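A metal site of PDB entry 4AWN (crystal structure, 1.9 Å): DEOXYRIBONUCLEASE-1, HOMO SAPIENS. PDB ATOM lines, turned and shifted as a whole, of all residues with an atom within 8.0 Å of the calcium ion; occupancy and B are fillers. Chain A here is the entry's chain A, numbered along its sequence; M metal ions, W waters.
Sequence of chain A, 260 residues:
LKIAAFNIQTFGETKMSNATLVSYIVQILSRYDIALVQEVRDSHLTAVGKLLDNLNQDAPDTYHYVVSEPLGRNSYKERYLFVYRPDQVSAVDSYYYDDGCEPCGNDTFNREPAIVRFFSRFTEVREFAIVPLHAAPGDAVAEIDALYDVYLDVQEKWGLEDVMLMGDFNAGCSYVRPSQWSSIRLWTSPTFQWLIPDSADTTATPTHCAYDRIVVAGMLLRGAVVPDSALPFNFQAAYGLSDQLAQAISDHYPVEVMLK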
ATOM      1  N   LEU A  71     -15.075   3.044 -27.813  1.00  0.00           N
ATOM      2  CA  LEU A  71     -13.688   2.562 -27.725  1.00  0.00           C
ATOM      3  C   LEU A  71     -13.521   1.580 -26.578  1.00  0.00           C
ATOM      4  O   LEU A  71     -14.163   1.704 -25.535  1.00  0.00           O
ATOM      5  CB  LEU A  71     -12.716   3.743 -27.517  1.00  0.00           C
ATOM      6  CG  LEU A  71     -12.652   4.721 -28.709  1.00  0.00           C
ATOM      7  CD1 LEU A  71     -12.061   6.102 -28.350  1.00  0.00           C
ATOM      8  CD2 LEU A  71     -11.862   4.065 -29.870  1.00  0.00           C
ATOM      9  N   GLY A  72     -12.639   0.611 -26.761  1.00  0.00           N
ATOM     10  CA  GLY A  72     -12.395  -0.405 -25.741  1.00  0.00           C
ATOM     11  C   GLY A  72     -12.103  -1.737 -26.408  1.00  0.00           C
ATOM     12  O   GLY A  72     -12.588  -1.992 -27.498  1.00  0.00           O
ATOM     13  N   ARG A  73     -11.304  -2.569 -25.759  1.00  0.00           N
ATOM     14  CA  ARG A  73     -10.892  -3.838 -26.363  1.00  0.00           C
ATOM     15  C   ARG A  73     -12.016  -4.900 -26.404  1.00  0.00           C
ATOM     16  O   ARG A  73     -11.994  -5.814 -27.255  1.00  0.00           O
ATOM     17  CB  ARG A  73      -9.637  -4.389 -25.687  1.00  0.00           C
ATOM     18  CG  ARG A  73      -8.504  -3.392 -25.629  1.00  0.00           C
ATOM     19  CD  ARG A  73      -7.197  -4.099 -25.672  1.00  0.00           C
ATOM     20  NE  ARG A  73      -6.057  -3.204 -25.565  1.00  0.00           N
ATOM     21  CZ  ARG A  73      -5.502  -2.822 -24.423  1.00  0.00           C
ATOM     22  NH1 ARG A  73      -6.022  -3.237 -23.255  1.00  0.00           N
ATOM     23  NH2 ARG A  73      -4.441  -2.027 -24.432  1.00  0.00           N
ATOM     24  N   TYR A  97      -6.054   8.431 -32.271  1.00  0.00           N
ATOM     25  CA  TYR A  97      -4.654   8.035 -32.133  1.00  0.00           C
ATOM     26  C   TYR A  97      -4.464   6.576 -32.536  1.00  0.00           C
ATOM     27  O   TYR A  97      -5.275   5.739 -32.164  1.00  0.00           O
ATOM     28  CB  TYR A  97      -4.160   8.244 -30.691  1.00  0.00           C
ATOM     29  CG  TYR A  97      -2.748   7.754 -30.494  1.00  0.00           C
ATOM     30  CD1 TYR A  97      -1.641   8.491 -30.985  1.00  0.00           C
ATOM     31  CD2 TYR A  97      -2.498   6.581 -29.806  1.00  0.00           C
ATOM     32  CE1 TYR A  97      -0.359   8.052 -30.794  1.00  0.00           C
ATOM     33  CE2 TYR A  97      -1.169   6.117 -29.625  1.00  0.00           C
ATOM     34  CZ  TYR A  97      -0.122   6.864 -30.118  1.00  0.00           C
ATOM     35  OH  TYR A  97       1.158   6.431 -29.939  1.00  0.00           O
ATOM     36  N   ASP A  98      -3.407   6.307 -33.317  1.00  0.00           N
ATOM     37  CA  ASP A  98      -3.013   4.953 -33.744  1.00  0.00           C
ATOM     38  C   ASP A  98      -2.153   4.344 -32.645  1.00  0.00           C
ATOM     39  O   ASP A  98      -0.968   4.660 -32.520  1.00  0.00           O
ATOM     40  CB  ASP A  98      -2.243   4.998 -35.084  1.00  0.00           C
ATOM     41  CG  ASP A  98      -1.606   3.643 -35.488  1.00  0.00           C
ATOM     42  OD1 ASP A  98      -2.029   2.574 -34.963  1.00  0.00           O
ATOM     43  OD2 ASP A  98      -0.668   3.637 -36.340  1.00  0.00           O
ATOM     44  N   ASP A  99      -2.771   3.487 -31.837  1.00  0.00           N
ATOM     45  CA  ASP A  99      -2.066   2.869 -30.694  1.00  0.00           C
ATOM     46  C   ASP A  99      -1.470   1.486 -31.041  1.00  0.00           C
ATOM     47  O   ASP A  99      -1.165   0.684 -30.156  1.00  0.00           O
ATOM     48  CB  ASP A  99      -2.965   2.841 -29.428  1.00  0.00           C
ATOM     49  CG  ASP A  99      -4.124   1.856 -29.532  1.00  0.00           C
ATOM     50  OD1 ASP A  99      -4.671   1.613 -30.615  1.00  0.00           O
ATOM     51  OD2 ASP A  99      -4.497   1.285 -28.492  1.00  0.00           O
ATOM     52  N   GLY A 100      -1.262   1.237 -32.336  1.00  0.00           N
ATOM     53  CA  GLY A 100      -0.701  -0.031 -32.776  1.00  0.00           C
ATOM     54  C   GLY A 100      -1.775  -1.031 -33.139  1.00  0.00           C
ATOM     55  O   GLY A 100      -2.877  -0.656 -33.533  1.00  0.00           O
ATOM     56  N   CYS A 101      -1.475  -2.307 -32.976  1.00  0.00           N
ATOM     57  CA  CYS A 101      -2.294  -3.376 -33.578  1.00  0.00           C
ATOM     58  C   CYS A 101      -3.269  -4.065 -32.614  1.00  0.00           C
ATOM     59  O   CYS A 101      -2.858  -4.926 -31.840  1.00  0.00           O
ATOM     60  CB  CYS A 101      -1.353  -4.389 -34.232  1.00  0.00           C
ATOM     61  SG  CYS A 101      -2.191  -5.692 -35.125  1.00  0.00           S
ATOM     62  N   GLU A 102      -4.560  -3.711 -32.669  1.00  0.00           N
ATOM     63  CA  GLU A 102      -5.553  -4.246 -31.714  1.00  0.00           C
ATOM     64  C   GLU A 102      -5.804  -5.742 -31.878  1.00  0.00           C
ATOM     65  O   GLU A 102      -5.657  -6.495 -30.910  1.00  0.00           O
ATOM     66  CB  GLU A 102      -6.900  -3.464 -31.703  1.00  0.00           C
ATOM     67  CG  GLU A 102      -7.772  -3.736 -30.436  1.00  0.00           C
ATOM     68  CD  GLU A 102      -9.085  -2.925 -30.386  1.00  0.00           C
ATOM     69  OE1 GLU A 102      -9.937  -3.105 -31.280  1.00  0.00           O
ATOM     70  OE2 GLU A 102      -9.282  -2.123 -29.432  1.00  0.00           O
ATOM     71  N   ASN A 106      -1.936  -6.160 -28.820  1.00  0.00           N
ATOM     72  CA  ASN A 106      -0.600  -5.568 -28.888  1.00  0.00           C
ATOM     73  C   ASN A 106      -0.656  -4.051 -28.613  1.00  0.00           C
ATOM     74  O   ASN A 106       0.349  -3.419 -28.256  1.00  0.00           O
ATOM     75  CB  ASN A 106      -0.176  -5.712 -30.333  1.00  0.00           C
ATOM     76  CG  ASN A 106       1.211  -6.215 -30.503  1.00  0.00           C
ATOM     77  OD1 ASN A 106       2.089  -6.025 -29.656  1.00  0.00           O
ATOM     78  ND2 ASN A 106       1.418  -6.855 -31.654  1.00  0.00           N
ATOM     79  N   ASP A 107      -1.840  -3.491 -28.807  1.00  0.00           N
ATOM     80  CA  ASP A 107      -2.070  -2.051 -28.872  1.00  0.00           C
ATOM     81  C   ASP A 107      -1.871  -1.403 -27.508  1.00  0.00           C
ATOM     82  O   ASP A 107      -2.020  -2.074 -26.483  1.00  0.00           O
ATOM     83  CB  ASP A 107      -3.476  -1.812 -29.347  1.00  0.00           C
ATOM     84  CG  ASP A 107      -4.502  -2.395 -28.415  1.00  0.00           C
ATOM     85  OD1 ASP A 107      -4.612  -3.637 -28.345  1.00  0.00           O
ATOM     86  OD2 ASP A 107      -5.181  -1.625 -27.718  1.00  0.00           O
ATOM     87  N   THR A 108      -1.530  -0.115 -27.492  1.00  0.00           N
ATOM     88  CA  THR A 108      -1.089   0.500 -26.249  1.00  0.00           C
ATOM     89  C   THR A 108      -2.176   1.066 -25.330  1.00  0.00           C
ATOM     90  O   THR A 108      -1.910   1.266 -24.144  1.00  0.00           O
ATOM     91  CB  THR A 108       0.043   1.531 -26.471  1.00  0.00           C
ATOM     92  OG1 THR A 108      -0.321   2.447 -27.523  1.00  0.00           O
ATOM     93  CG2 THR A 108       1.320   0.810 -26.849  1.00  0.00           C
ATOM     94  N   PHE A 109      -3.379   1.336 -25.846  1.00  0.00           N
ATOM     95  CA  PHE A 109      -4.442   1.888 -24.991  1.00  0.00           C
ATOM     96  C   PHE A 109      -5.695   1.023 -25.036  1.00  0.00           C
ATOM     97  O   PHE A 109      -6.082   0.554 -26.086  1.00  0.00           O
ATOM     98  CB  PHE A 109      -4.855   3.310 -25.447  1.00  0.00           C
ATOM     99  CG  PHE A 109      -3.820   4.355 -25.206  1.00  0.00           C
ATOM    100  CD1 PHE A 109      -3.720   4.973 -23.948  1.00  0.00           C
ATOM    101  CD2 PHE A 109      -2.950   4.768 -26.233  1.00  0.00           C
ATOM    102  CE1 PHE A 109      -2.772   5.947 -23.701  1.00  0.00           C
ATOM    103  CE2 PHE A 109      -1.970   5.740 -26.007  1.00  0.00           C
ATOM    104  CZ  PHE A 109      -1.896   6.353 -24.725  1.00  0.00           C
ATOM    105  N   ASN A 110      -6.353   0.852 -23.899  1.00  0.00           N
ATOM    106  CA  ASN A 110      -7.709   0.322 -23.918  1.00  0.00           C
ATOM    107  C   ASN A 110      -8.620   1.264 -24.720  1.00  0.00           C
ATOM    108  O   ASN A 110      -9.332   0.836 -25.648  1.00  0.00           O
ATOM    109  CB  ASN A 110      -8.234   0.160 -22.494  1.00  0.00           C
ATOM    110  CG  ASN A 110      -9.336  -0.862 -22.405  1.00  0.00           C
ATOM    111  OD1 ASN A 110     -10.325  -0.795 -23.134  1.00  0.00           O
ATOM    112  ND2 ASN A 110      -9.176  -1.814 -21.485  1.00  0.00           N
ATOM    113  N   ARG A 111      -8.578   2.559 -24.369  1.00  0.00           N
ATOM    114  CA  ARG A 111      -9.400   3.572 -25.045  1.00  0.00           C
ATOM    115  C   ARG A 111      -8.472   4.644 -25.592  1.00  0.00           C
ATOM    116  O   ARG A 111      -8.302   5.697 -24.974  1.00  0.00           O
ATOM    117  CB  ARG A 111     -10.410   4.188 -24.055  1.00  0.00           C
ATOM    118  CG  ARG A 111     -11.502   3.192 -23.575  1.00  0.00           C
ATOM    119  CD  ARG A 111     -12.225   3.707 -22.314  1.00  0.00           C
ATOM    120  NE  ARG A 111     -11.366   3.615 -21.126  1.00  0.00           N
ATOM    121  CZ  ARG A 111     -11.370   2.603 -20.252  1.00  0.00           C
ATOM    122  NH1 ARG A 111     -12.213   1.574 -20.415  1.00  0.00           N
ATOM    123  NH2 ARG A 111     -10.545   2.602 -19.206  1.00  0.00           N
ATOM    124  N   GLU A 112      -7.868   4.349 -26.741  1.00  0.00           N
ATOM    125  CA  GLU A 112      -6.917   5.280 -27.366  1.00  0.00           C
ATOM    126  C   GLU A 112      -7.590   6.625 -27.552  1.00  0.00           C
ATOM    127  O   GLU A 112      -8.786   6.705 -27.847  1.00  0.00           O
ATOM    128  CB  GLU A 112      -6.378   4.755 -28.704  1.00  0.00           C
ATOM    129  CG  GLU A 112      -7.402   4.286 -29.727  1.00  0.00           C
ATOM    130  CD  GLU A 112      -7.879   2.850 -29.497  1.00  0.00           C
ATOM    131  OE1 GLU A 112      -7.367   2.140 -28.590  1.00  0.00           O
ATOM    132  OE2 GLU A 112      -8.804   2.432 -30.233  1.00  0.00           O
ATOM    133  N   PRO A 113      -6.833   7.700 -27.333  1.00  0.00           N
ATOM    134  CA  PRO A 113      -7.432   9.024 -27.345  1.00  0.00           C
ATOM    135  C   PRO A 113      -8.101   9.385 -28.688  1.00  0.00           C
ATOM    136  O   PRO A 113      -7.547   9.099 -29.748  1.00  0.00           O
ATOM    137  CB  PRO A 113      -6.250   9.940 -27.064  1.00  0.00           C
ATOM    138  CG  PRO A 113      -5.293   9.099 -26.257  1.00  0.00           C
ATOM    139  CD  PRO A 113      -5.425   7.725 -26.885  1.00  0.00           C
ATOM    140  N   GLU A 143      -0.107   3.343 -19.823  1.00  0.00           N
ATOM    141  CA  GLU A 143      -0.979   4.191 -20.633  1.00  0.00           C
ATOM    142  C   GLU A 143      -0.633   5.664 -20.461  1.00  0.00           C
ATOM    143  O   GLU A 143      -0.475   6.396 -21.453  1.00  0.00           O
ATOM    144  CB  GLU A 143      -2.458   3.880 -20.376  1.00  0.00           C
ATOM    145  CG  GLU A 143      -2.873   2.573 -21.026  1.00  0.00           C
ATOM    146  CD  GLU A 143      -4.370   2.362 -21.104  1.00  0.00           C
ATOM    147  OE1 GLU A 143      -5.140   3.230 -20.671  1.00  0.00           O
ATOM    148  OE2 GLU A 143      -4.793   1.296 -21.627  1.00  0.00           O
HETATM  149 CA    CA M   1      -6.333   0.174 -28.173  1.00  0.00          CA
HETATM  150  O   HOH W   1      -8.182  -0.733 -27.688  1.00  0.00           O
HETATM  151  O   HOH W   2      -6.453  -0.404 -30.396  1.00  0.00           O
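O of Asn 110 lies close to N of Gly 72 (3.5 Å).
N of Arg 73 is in hydrogen-bond range of OD1 of Asn 110 (3.3 Å).
O of Asp 99 sits at hydrogen-bond distance from N of Thr 108, at 2.8 Å.
OD1 of Asp 107 lies within salt-bridge range of NE of Arg 73 (3.2 Å).
O of Phe 109 sits close to NH2 of Arg 73 (3.5 Å).
The backbone NH (N) of Asn 110 lies within hydrogen-bond range of the side-chain carboxylate (OE2) of Glu 143, at 2.8 Å.
Glu 102 touches the calcium ion (OE2 to CA, 3.9 Å).
Asn 110 touches the calcium ion (O to CA, 3.98 Å).
Of the 18 residues printed, 6 come within 4 Å of the calcium ion.
Along chain A the residues within 4 Å of the calcium ion span positions 99 to 112.
The nearest printed residue that does not touch the calcium ion is Arg 73 (4.3 Å).
The calcium ion is bound by water W1 (2.1 Å), the backbone carbonyl oxygen of Phe 109 (2.1 Å), the side-chain carboxylate of Asp 99 (2.2 Å), the side-chain carboxylate of Asp 107 (2.2 Å), the side-chain carboxylate of Glu 112 (2.3 Å) and water W2 (2.3 Å).
Water W1 bridges the side-chain carboxylate of Glu 102 (2.5 Å) and the backbone carbonyl oxygen of Asn 110 (2.8 Å).
Water W2 bridges OD1 of Asp 99 (2.7 Å) and OE2 of Glu 102 (3.4 Å).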
